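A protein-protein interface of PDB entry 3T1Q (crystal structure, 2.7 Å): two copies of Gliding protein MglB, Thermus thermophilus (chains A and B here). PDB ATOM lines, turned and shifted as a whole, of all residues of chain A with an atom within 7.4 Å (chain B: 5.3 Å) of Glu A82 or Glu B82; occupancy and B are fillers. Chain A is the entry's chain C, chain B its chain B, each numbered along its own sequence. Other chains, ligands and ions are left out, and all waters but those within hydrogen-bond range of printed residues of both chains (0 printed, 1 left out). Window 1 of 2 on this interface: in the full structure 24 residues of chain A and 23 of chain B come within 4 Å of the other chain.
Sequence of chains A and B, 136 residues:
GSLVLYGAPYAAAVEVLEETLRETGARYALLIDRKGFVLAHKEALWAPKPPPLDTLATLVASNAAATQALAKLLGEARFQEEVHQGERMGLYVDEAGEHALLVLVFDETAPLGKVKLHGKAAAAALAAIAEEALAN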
ATOM      1  N   VAL A  60     -12.691   8.168 -15.354  1.00  0.00           N
ATOM      2  CA  VAL A  60     -11.966   7.248 -16.224  1.00  0.00           C
ATOM      3  C   VAL A  60     -11.240   7.923 -17.429  1.00  0.00           C
ATOM      4  O   VAL A  60     -10.176   7.464 -17.844  1.00  0.00           O
ATOM      5  CB  VAL A  60     -12.906   6.093 -16.695  1.00  0.00           C
ATOM      6  CG1 VAL A  60     -12.249   5.226 -17.802  1.00  0.00           C
ATOM      7  CG2 VAL A  60     -13.294   5.274 -15.509  1.00  0.00           C
ATOM      8  N   ASN A  63      -8.136   9.556 -15.799  1.00  0.00           N
ATOM      9  CA  ASN A  63      -7.240   8.509 -15.408  1.00  0.00           C
ATOM     10  C   ASN A  63      -6.503   7.973 -16.658  1.00  0.00           C
ATOM     11  O   ASN A  63      -5.283   7.720 -16.636  1.00  0.00           O
ATOM     12  CB  ASN A  63      -8.100   7.454 -14.705  1.00  0.00           C
ATOM     13  CG  ASN A  63      -7.397   6.128 -14.493  1.00  0.00           C
ATOM     14  OD1 ASN A  63      -6.236   6.080 -14.060  1.00  0.00           O
ATOM     15  ND2 ASN A  63      -8.117   5.018 -14.796  1.00  0.00           N
ATOM     16  N   ALA A  64      -7.220   7.820 -17.762  1.00  0.00           N
ATOM     17  CA  ALA A  64      -6.569   7.370 -18.982  1.00  0.00           C
ATOM     18  C   ALA A  64      -5.652   8.433 -19.539  1.00  0.00           C
ATOM     19  O   ALA A  64      -4.664   8.121 -20.188  1.00  0.00           O
ATOM     20  CB  ALA A  64      -7.574   7.017 -20.000  1.00  0.00           C
ATOM     21  N   THR A  67      -2.423   8.641 -17.291  1.00  0.00           N
ATOM     22  CA  THR A  67      -1.471   7.529 -17.404  1.00  0.00           C
ATOM     23  C   THR A  67      -0.857   7.503 -18.773  1.00  0.00           C
ATOM     24  O   THR A  67       0.318   7.195 -18.930  1.00  0.00           O
ATOM     25  CB  THR A  67      -2.072   6.158 -17.095  1.00  0.00           C
ATOM     26  OG1 THR A  67      -3.177   5.944 -17.963  1.00  0.00           O
ATOM     27  CG2 THR A  67      -2.537   6.064 -15.621  1.00  0.00           C
ATOM     28  N   ARG A  78       2.219   3.760 -25.169  1.00  0.00           N
ATOM     29  CA  ARG A  78       1.107   3.495 -24.285  1.00  0.00           C
ATOM     30  C   ARG A  78       1.460   2.485 -23.200  1.00  0.00           C
ATOM     31  O   ARG A  78       2.421   1.740 -23.319  1.00  0.00           O
ATOM     32  CB  ARG A  78      -0.122   3.046 -25.098  1.00  0.00           C
ATOM     33  CG  ARG A  78      -0.331   1.530 -25.258  1.00  0.00           C
ATOM     34  CD  ARG A  78      -1.765   1.322 -25.686  1.00  0.00           C
ATOM     35  NE  ARG A  78      -2.364   0.030 -25.342  1.00  0.00           N
ATOM     36  CZ  ARG A  78      -3.370  -0.128 -24.488  1.00  0.00           C
ATOM     37  NH1 ARG A  78      -3.858   0.916 -23.840  1.00  0.00           N
ATOM     38  NH2 ARG A  78      -3.866  -1.338 -24.266  1.00  0.00           N
ATOM     39  N   PHE A  79       0.691   2.519 -22.117  1.00  0.00           N
ATOM     40  CA  PHE A  79       0.742   1.457 -21.113  1.00  0.00           C
ATOM     41  C   PHE A  79      -0.269   0.349 -21.528  1.00  0.00           C
ATOM     42  O   PHE A  79      -1.022   0.491 -22.512  1.00  0.00           O
ATOM     43  CB  PHE A  79       0.437   1.996 -19.712  1.00  0.00           C
ATOM     44  CG  PHE A  79       1.570   2.791 -19.084  1.00  0.00           C
ATOM     45  CD1 PHE A  79       2.903   2.353 -19.162  1.00  0.00           C
ATOM     46  CD2 PHE A  79       1.302   3.962 -18.360  1.00  0.00           C
ATOM     47  CE1 PHE A  79       3.925   3.068 -18.549  1.00  0.00           C
ATOM     48  CE2 PHE A  79       2.342   4.681 -17.742  1.00  0.00           C
ATOM     49  CZ  PHE A  79       3.641   4.227 -17.839  1.00  0.00           C
ATOM     50  N   GLN A  80      -0.268  -0.766 -20.822  1.00  0.00           N
ATOM     51  CA  GLN A  80      -1.244  -1.791 -21.110  1.00  0.00           C
ATOM     52  C   GLN A  80      -2.643  -1.436 -20.557  1.00  0.00           C
ATOM     53  O   GLN A  80      -2.810  -0.459 -19.834  1.00  0.00           O
ATOM     54  CB  GLN A  80      -0.742  -3.144 -20.582  1.00  0.00           C
ATOM     55  CG  GLN A  80      -0.265  -4.077 -21.682  1.00  0.00           C
ATOM     56  CD  GLN A  80       1.179  -3.878 -21.998  1.00  0.00           C
ATOM     57  OE1 GLN A  80       2.030  -4.677 -21.558  1.00  0.00           O
ATOM     58  NE2 GLN A  80       1.497  -2.802 -22.755  1.00  0.00           N
ATOM     59  N   GLU A  81      -3.650  -2.221 -20.911  1.00  0.00           N
ATOM     60  CA  GLU A  81      -4.995  -2.027 -20.362  1.00  0.00           C
ATOM     61  C   GLU A  81      -4.973  -2.027 -18.852  1.00  0.00           C
ATOM     62  O   GLU A  81      -4.202  -2.742 -18.248  1.00  0.00           O
ATOM     63  CB  GLU A  81      -5.960  -3.098 -20.864  1.00  0.00           C
ATOM     64  CG  GLU A  81      -5.746  -4.467 -20.308  1.00  0.00           C
ATOM     65  CD  GLU A  81      -4.797  -5.323 -21.120  1.00  0.00           C
ATOM     66  OE1 GLU A  81      -4.278  -4.913 -22.210  1.00  0.00           O
ATOM     67  OE2 GLU A  81      -4.576  -6.453 -20.640  1.00  0.00           O
ATOM     68  N   GLU A  82      -5.825  -1.233 -18.232  1.00  0.00           N
ATOM     69  CA  GLU A  82      -5.843  -1.178 -16.784  1.00  0.00           C
ATOM     70  C   GLU A  82      -6.976  -1.988 -16.133  1.00  0.00           C
ATOM     71  O   GLU A  82      -8.118  -1.969 -16.609  1.00  0.00           O
ATOM     72  CB  GLU A  82      -5.930   0.274 -16.341  1.00  0.00           C
ATOM     73  CG  GLU A  82      -5.506   0.477 -14.928  1.00  0.00           C
ATOM     74  CD  GLU A  82      -4.734   1.756 -14.781  1.00  0.00           C
ATOM     75  OE1 GLU A  82      -5.102   2.740 -15.507  1.00  0.00           O
ATOM     76  OE2 GLU A  82      -3.770   1.764 -13.942  1.00  0.00           O
ATOM     77  N   VAL A  83      -6.638  -2.683 -15.047  1.00  0.00           N
ATOM     78  CA  VAL A  83      -7.614  -3.253 -14.146  1.00  0.00           C
ATOM     79  C   VAL A  83      -7.399  -2.627 -12.780  1.00  0.00           C
ATOM     80  O   VAL A  83      -6.297  -2.677 -12.251  1.00  0.00           O
ATOM     81  CB  VAL A  83      -7.441  -4.780 -13.992  1.00  0.00           C
ATOM     82  CG1 VAL A  83      -8.556  -5.386 -13.117  1.00  0.00           C
ATOM     83  CG2 VAL A  83      -7.378  -5.474 -15.354  1.00  0.00           C
ATOM     84  N   HIS A  84      -8.446  -2.023 -12.220  1.00  0.00           N
ATOM     85  CA  HIS A  84      -8.436  -1.580 -10.834  1.00  0.00           C
ATOM     86  C   HIS A  84      -9.290  -2.517 -10.027  1.00  0.00           C
ATOM     87  O   HIS A  84     -10.417  -2.820 -10.423  1.00  0.00           O
ATOM     88  CB  HIS A  84      -9.014  -0.201 -10.696  1.00  0.00           C
ATOM     89  CG  HIS A  84      -8.255   0.852 -11.430  1.00  0.00           C
ATOM     90  ND1 HIS A  84      -8.790   1.542 -12.503  1.00  0.00           N
ATOM     91  CD2 HIS A  84      -7.015   1.353 -11.233  1.00  0.00           C
ATOM     92  CE1 HIS A  84      -7.906   2.419 -12.940  1.00  0.00           C
ATOM     93  NE2 HIS A  84      -6.826   2.330 -12.180  1.00  0.00           N
ATOM     94  N   LEU A  91     -12.771  -2.258 -12.015  1.00  0.00           N
ATOM     95  CA  LEU A  91     -12.954  -1.628 -13.350  1.00  0.00           C
ATOM     96  C   LEU A  91     -11.983  -2.209 -14.319  1.00  0.00           C
ATOM     97  O   LEU A  91     -10.877  -2.491 -13.942  1.00  0.00           O
ATOM     98  CB  LEU A  91     -12.665  -0.149 -13.333  1.00  0.00           C
ATOM     99  CG  LEU A  91     -13.687   0.815 -12.815  1.00  0.00           C
ATOM    100  CD1 LEU A  91     -13.805   0.412 -11.382  1.00  0.00           C
ATOM    101  CD2 LEU A  91     -13.186   2.277 -12.907  1.00  0.00           C
ATOM    102  N   TYR A  92     -12.403  -2.381 -15.561  1.00  0.00           N
ATOM    103  CA  TYR A  92     -11.501  -2.740 -16.639  1.00  0.00           C
ATOM    104  C   TYR A  92     -11.666  -1.679 -17.704  1.00  0.00           C
ATOM    105  O   TYR A  92     -12.801  -1.464 -18.195  1.00  0.00           O
ATOM    106  CB  TYR A  92     -11.834  -4.117 -17.222  1.00  0.00           C
ATOM    107  CG  TYR A  92     -11.116  -4.487 -18.506  1.00  0.00           C
ATOM    108  CD1 TYR A  92     -10.006  -5.342 -18.488  1.00  0.00           C
ATOM    109  CD2 TYR A  92     -11.545  -4.019 -19.732  1.00  0.00           C
ATOM    110  CE1 TYR A  92      -9.337  -5.718 -19.647  1.00  0.00           C
ATOM    111  CE2 TYR A  92     -10.882  -4.383 -20.921  1.00  0.00           C
ATOM    112  CZ  TYR A  92      -9.772  -5.233 -20.857  1.00  0.00           C
ATOM    113  OH  TYR A  92      -9.098  -5.580 -22.009  1.00  0.00           O
ATOM    114  N   VAL A  93     -10.537  -1.040 -18.054  1.00  0.00           N
ATOM    115  CA  VAL A  93     -10.460   0.034 -19.057  1.00  0.00           C
ATOM    116  C   VAL A  93      -9.450  -0.311 -20.143  1.00  0.00           C
ATOM    117  O   VAL A  93      -8.318  -0.602 -19.857  1.00  0.00           O
ATOM    118  CB  VAL A  93      -9.975   1.365 -18.424  1.00  0.00           C
ATOM    119  CG1 VAL A  93     -10.114   2.515 -19.409  1.00  0.00           C
ATOM    120  CG2 VAL A  93     -10.719   1.661 -17.184  1.00  0.00           C
ATOM    121  N   ASP A  94      -9.842  -0.231 -21.395  1.00  0.00           N
ATOM    122  CA  ASP A  94      -8.947  -0.531 -22.477  1.00  0.00           C
ATOM    123  C   ASP A  94      -9.239   0.393 -23.676  1.00  0.00           C
ATOM    124  O   ASP A  94     -10.178   1.168 -23.660  1.00  0.00           O
ATOM    125  CB  ASP A  94      -9.130  -1.987 -22.811  1.00  0.00           C
ATOM    126  CG  ASP A  94      -8.075  -2.516 -23.724  1.00  0.00           C
ATOM    127  OD1 ASP A  94      -7.098  -1.807 -24.061  1.00  0.00           O
ATOM    128  OD2 ASP A  94      -8.236  -3.681 -24.101  1.00  0.00           O
ATOM    129  N   GLU A  95      -8.401   0.355 -24.702  1.00  0.00           N
ATOM    130  CA  GLU A  95      -8.510   1.322 -25.782  1.00  0.00           C
ATOM    131  C   GLU A  95      -9.436   0.826 -26.866  1.00  0.00           C
ATOM    132  O   GLU A  95      -9.296  -0.288 -27.351  1.00  0.00           O
ATOM    133  CB  GLU A  95      -7.127   1.711 -26.338  1.00  0.00           C
ATOM    134  CG  GLU A  95      -6.421   2.743 -25.457  1.00  0.00           C
ATOM    135  CD  GLU A  95      -4.986   3.167 -25.892  1.00  0.00           C
ATOM    136  OE1 GLU A  95      -4.495   2.800 -26.990  1.00  0.00           O
ATOM    137  OE2 GLU A  95      -4.347   3.898 -25.086  1.00  0.00           O
ATOM    138  N   LEU A 102     -13.118   1.544 -23.802  1.00  0.00           N
ATOM    139  CA  LEU A 102     -14.081   0.603 -23.261  1.00  0.00           C
ATOM    140  C   LEU A 102     -13.994   0.609 -21.736  1.00  0.00           C
ATOM    141  O   LEU A 102     -12.921   0.383 -21.175  1.00  0.00           O
ATOM    142  CB  LEU A 102     -13.777  -0.801 -23.746  1.00  0.00           C
ATOM    143  CG  LEU A 102     -14.744  -1.827 -23.119  1.00  0.00           C
ATOM    144  CD1 LEU A 102     -16.063  -1.787 -23.810  1.00  0.00           C
ATOM    145  CD2 LEU A 102     -14.193  -3.207 -23.167  1.00  0.00           C
ATOM    146  N   LEU A 104     -15.606  -1.389 -18.396  1.00  0.00           N
ATOM    147  CA  LEU A 104     -16.503  -2.370 -17.769  1.00  0.00           C
ATOM    148  C   LEU A 104     -16.467  -2.267 -16.229  1.00  0.00           C
ATOM    149  O   LEU A 104     -15.382  -2.303 -15.636  1.00  0.00           O
ATOM    150  CB  LEU A 104     -16.075  -3.765 -18.146  1.00  0.00           C
ATOM    151  CG  LEU A 104     -15.961  -4.247 -19.571  1.00  0.00           C
ATOM    152  CD1 LEU A 104     -15.402  -5.661 -19.477  1.00  0.00           C
ATOM    153  CD2 LEU A 104     -17.279  -4.304 -20.203  1.00  0.00           C
ATOM    154  N   PHE A 106     -17.373  -4.204 -12.733  1.00  0.00           N
ATOM    155  CA  PHE A 106     -17.691  -5.550 -12.297  1.00  0.00           C
ATOM    156  C   PHE A 106     -17.537  -5.755 -10.808  1.00  0.00           C
ATOM    157  O   PHE A 106     -16.963  -4.911 -10.120  1.00  0.00           O
ATOM    158  CB  PHE A 106     -16.852  -6.575 -13.064  1.00  0.00           C
ATOM    159  CG  PHE A 106     -15.356  -6.426 -12.874  1.00  0.00           C
ATOM    160  CD1 PHE A 106     -14.675  -7.201 -11.914  1.00  0.00           C
ATOM    161  CD2 PHE A 106     -14.617  -5.558 -13.688  1.00  0.00           C
ATOM    162  CE1 PHE A 106     -13.269  -7.088 -11.730  1.00  0.00           C
ATOM    163  CE2 PHE A 106     -13.220  -5.438 -13.534  1.00  0.00           C
ATOM    164  CZ  PHE A 106     -12.547  -6.199 -12.537  1.00  0.00           C
ATOM    165  N   ASN B  63      -3.247  11.471 -10.938  1.00  0.00           N
ATOM    166  CA  ASN B  63      -3.782  10.184 -11.211  1.00  0.00           C
ATOM    167  C   ASN B  63      -4.336   9.547  -9.952  1.00  0.00           C
ATOM    168  O   ASN B  63      -5.389   8.921  -9.999  1.00  0.00           O
ATOM    169  CB  ASN B  63      -2.756   9.303 -11.850  1.00  0.00           C
ATOM    170  CG  ASN B  63      -3.397   8.167 -12.569  1.00  0.00           C
ATOM    171  OD1 ASN B  63      -4.410   8.364 -13.287  1.00  0.00           O
ATOM    172  ND2 ASN B  63      -2.867   6.950 -12.358  1.00  0.00           N
ATOM    173  N   ALA B  64      -3.653   9.737  -8.829  1.00  0.00           N
ATOM    174  CA  ALA B  64      -4.072   9.132  -7.588  1.00  0.00           C
ATOM    175  C   ALA B  64      -5.366   9.760  -7.116  1.00  0.00           C
ATOM    176  O   ALA B  64      -6.240   9.068  -6.580  1.00  0.00           O
ATOM    177  CB  ALA B  64      -3.021   9.255  -6.566  1.00  0.00           C
ATOM    178  N   THR B  67      -8.181   7.964  -9.322  1.00  0.00           N
ATOM    179  CA  THR B  67      -8.428   6.598  -8.901  1.00  0.00           C
ATOM    180  C   THR B  67      -8.940   6.472  -7.478  1.00  0.00           C
ATOM    181  O   THR B  67      -9.764   5.577  -7.267  1.00  0.00           O
ATOM    182  CB  THR B  67      -7.253   5.661  -9.145  1.00  0.00           C
ATOM    183  OG1 THR B  67      -6.161   6.062  -8.350  1.00  0.00           O
ATOM    184  CG2 THR B  67      -6.822   5.743 -10.592  1.00  0.00           C
ATOM    185  N   GLN B  80      -5.736  -1.442  -5.247  1.00  0.00           N
ATOM    186  CA  GLN B  80      -4.399  -1.767  -4.762  1.00  0.00           C
ATOM    187  C   GLN B  80      -3.256  -0.986  -5.448  1.00  0.00           C
ATOM    188  O   GLN B  80      -3.508  -0.004  -6.145  1.00  0.00           O
ATOM    189  CB  GLN B  80      -4.168  -3.272  -4.801  1.00  0.00           C
ATOM    190  CG  GLN B  80      -4.247  -3.914  -6.153  1.00  0.00           C
ATOM    191  CD  GLN B  80      -4.874  -5.256  -6.006  1.00  0.00           C
ATOM    192  OE1 GLN B  80      -5.633  -5.462  -5.050  1.00  0.00           O
ATOM    193  NE2 GLN B  80      -4.571  -6.193  -6.920  1.00  0.00           N
ATOM    194  N   GLU B  81      -2.009  -1.395  -5.224  1.00  0.00           N
ATOM    195  CA  GLU B  81      -0.866  -0.766  -5.894  1.00  0.00           C
ATOM    196  C   GLU B  81      -0.992  -0.991  -7.389  1.00  0.00           C
ATOM    197  O   GLU B  81      -1.554  -2.006  -7.809  1.00  0.00           O
ATOM    198  CB  GLU B  81       0.483  -1.328  -5.417  1.00  0.00           C
ATOM    199  CG  GLU B  81       0.457  -2.310  -4.256  1.00  0.00           C
ATOM    200  CD  GLU B  81       0.172  -3.758  -4.689  1.00  0.00           C
ATOM    201  OE1 GLU B  81       0.731  -4.196  -5.744  1.00  0.00           O
ATOM    202  OE2 GLU B  81      -0.614  -4.445  -3.965  1.00  0.00           O
ATOM    203  N   GLU B  82      -0.458  -0.043  -8.165  1.00  0.00           N
ATOM    204  CA  GLU B  82      -0.497  -0.061  -9.629  1.00  0.00           C
ATOM    205  C   GLU B  82       0.894  -0.331 -10.234  1.00  0.00           C
ATOM    206  O   GLU B  82       1.908   0.162  -9.749  1.00  0.00           O
ATOM    207  CB  GLU B  82      -1.076   1.258 -10.215  1.00  0.00           C
ATOM    208  CG  GLU B  82      -1.603   2.288  -9.184  1.00  0.00           C
ATOM    209  CD  GLU B  82      -2.540   3.361  -9.767  1.00  0.00           C
ATOM    210  OE1 GLU B  82      -2.774   3.320 -10.991  1.00  0.00           O
ATOM    211  OE2 GLU B  82      -3.044   4.246  -9.009  1.00  0.00           O
ATOM    212  N   VAL B  83       0.926  -1.102 -11.303  1.00  0.00           N
ATOM    213  CA  VAL B  83       2.146  -1.377 -12.024  1.00  0.00           C
ATOM    214  C   VAL B  83       1.799  -1.029 -13.435  1.00  0.00           C
ATOM    215  O   VAL B  83       0.946  -1.690 -13.988  1.00  0.00           O
ATOM    216  CB  VAL B  83       2.516  -2.900 -12.008  1.00  0.00           C
ATOM    217  CG1 VAL B  83       3.613  -3.239 -13.052  1.00  0.00           C
ATOM    218  CG2 VAL B  83       2.930  -3.314 -10.659  1.00  0.00           C
ATOM    219  N   HIS B  84       2.416  -0.002 -14.017  1.00  0.00           N
ATOM    220  CA  HIS B  84       2.166   0.266 -15.427  1.00  0.00           C
ATOM    221  C   HIS B  84       3.341  -0.186 -16.215  1.00  0.00           C
ATOM    222  O   HIS B  84       4.470   0.033 -15.821  1.00  0.00           O
ATOM    223  CB  HIS B  84       1.931   1.715 -15.713  1.00  0.00           C
ATOM    224  CG  HIS B  84       0.862   2.333 -14.882  1.00  0.00           C
ATOM    225  ND1 HIS B  84       1.137   3.096 -13.764  1.00  0.00           N
ATOM    226  CD2 HIS B  84      -0.481   2.334 -15.020  1.00  0.00           C
ATOM    227  CE1 HIS B  84       0.011   3.546 -13.246  1.00  0.00           C
ATOM    228  NE2 HIS B  84      -0.986   3.096 -13.991  1.00  0.00           N
ATOM    229  N   LEU B  91       6.465   1.517 -14.227  1.00  0.00           N
ATOM    230  CA  LEU B  91       6.193   2.433 -13.149  1.00  0.00           C
ATOM    231  C   LEU B  91       5.385   1.671 -12.113  1.00  0.00           C
ATOM    232  O   LEU B  91       4.408   0.974 -12.465  1.00  0.00           O
ATOM    233  CB  LEU B  91       5.352   3.539 -13.705  1.00  0.00           C
ATOM    234  CG  LEU B  91       5.319   4.884 -13.063  1.00  0.00           C
ATOM    235  CD1 LEU B  91       6.698   5.398 -12.842  1.00  0.00           C
ATOM    236  CD2 LEU B  91       4.596   5.780 -14.049  1.00  0.00           C
ATOM    237  N   TYR B  92       5.807   1.796 -10.849  1.00  0.00           N
ATOM    238  CA  TYR B  92       5.215   1.137  -9.692  1.00  0.00           C
ATOM    239  C   TYR B  92       4.741   2.229  -8.788  1.00  0.00           C
ATOM    240  O   TYR B  92       5.517   3.063  -8.408  1.00  0.00           O
ATOM    241  CB  TYR B  92       6.263   0.273  -8.947  1.00  0.00           C
ATOM    242  CG  TYR B  92       5.716  -0.393  -7.696  1.00  0.00           C
ATOM    243  CD1 TYR B  92       4.996  -1.613  -7.763  1.00  0.00           C
ATOM    244  CD2 TYR B  92       5.871   0.208  -6.452  1.00  0.00           C
ATOM    245  CE1 TYR B  92       4.461  -2.219  -6.601  1.00  0.00           C
ATOM    246  CE2 TYR B  92       5.346  -0.367  -5.291  1.00  0.00           C
ATOM    247  CZ  TYR B  92       4.644  -1.573  -5.361  1.00  0.00           C
ATOM    248  OH  TYR B  92       4.131  -2.091  -4.184  1.00  0.00           O
ATOM    249  N   VAL B  93       3.475   2.248  -8.426  1.00  0.00           N
ATOM    250  CA  VAL B  93       3.004   3.272  -7.499  1.00  0.00           C
ATOM    251  C   VAL B  93       2.298   2.645  -6.279  1.00  0.00           C
ATOM    252  O   VAL B  93       1.433   1.763  -6.431  1.00  0.00           O
ATOM    253  CB  VAL B  93       2.074   4.333  -8.236  1.00  0.00           C
ATOM    254  CG1 VAL B  93       1.435   5.300  -7.257  1.00  0.00           C
ATOM    255  CG2 VAL B  93       2.860   5.121  -9.246  1.00  0.00           C
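The side-chain amide oxygen (OD1) of Asn A63 sits close to the side-chain amide oxygen (OD1) of Asn B63.
A ring nitrogen (NE2) of His B84 is in hydrogen-bond range of the side-chain carboxylate (OE2) of Glu A82, 3.1 Å away.
The side-chain carboxylate (OE1) of Glu B82 sits close to the side-chain carboxylate (OE2) of Glu A82, 3.5 Å away.
The side-chain hydroxyl (OG1) of Thr B67 is in hydrogen-bond range of the backbone carbonyl oxygen (O) of Asn B63.
O of Ala B64 lies within hydrogen-bond range of OG1 of Thr B67 (3.5 Å).
O of Glu B82 sits at hydrogen-bond distance from N of Val B93, at 2.9 Å.
The backbone carbonyl oxygen (O) of Asn A63 is in hydrogen-bond range of the side-chain hydroxyl (OG1) of Thr A67, at 3.1 Å.
OG1 of Thr A67 is in hydrogen-bond range of O of Ala A64 (3.4 Å).
The backbone carbonyl oxygen (O) of His A84 lies within hydrogen-bond range of the backbone NH (N) of Leu A91 (2.9 Å).
Thr B67 touches Asn A63 (CG2 to OD1, 3.5 Å).
CG2 of Thr A67 touches ND2 of Asn B63, 3.4 Å away.
His B84 touches Thr A67 (NE2 to CG2, 3.7 Å).
His B84 touches Phe A79.
His A84 touches Thr B67 (NE2 to CG2, 3.8 Å).
Glu A82 touches just these residues of chain B: Glu B82 and His B84.
Of chain A, only Glu A82 (3.5 Å) comes within 4 Å of Glu B82.
Printed residues of chain A within 4 Å of Asn B63: Asn A63 and Thr A67.
Of the printed residues of chain B, Asn A63 touches Asn B63 and Thr B67.
Tyr B92 touches none of the printed residues of chain A.
The nearest residue of chain A that does not touch Glu B82 is His A84 (4.3 Å).
The nearest printed residue of chain A that does not touch Thr B67 is Glu A82 (6.0 Å).
Of the 11 printed residues of chain B, 4 touch a printed residue of chain A.
Hydrophobic or aromatic side chains of chain B that line the printed part of chain A: His B84.
Along chain B the printed residues that touch a printed residue of chain A span positions 63 to 84.
Among the printed residues, 8 pairs touch across the chains.
Among the printed residues, no Asp or Glu carboxylate lies within 4 Å of a Lys or Arg side-chain nitrogen of the other chain.
Asn B63 touches its own counterpart, Asn A63.
Thr A67 touches His B84, and with the chains exchanged His A84 touches Thr B67.
Glu B82 touches its own counterpart, Glu A82.
Glu A82 touches His B84, but with the chains exchanged His A84 does not touch Glu B82 (4.3 Å).
Of the 8 pairs that touch across the chains among the printed residues, 6 have their exchanged pair printed and touching as well.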
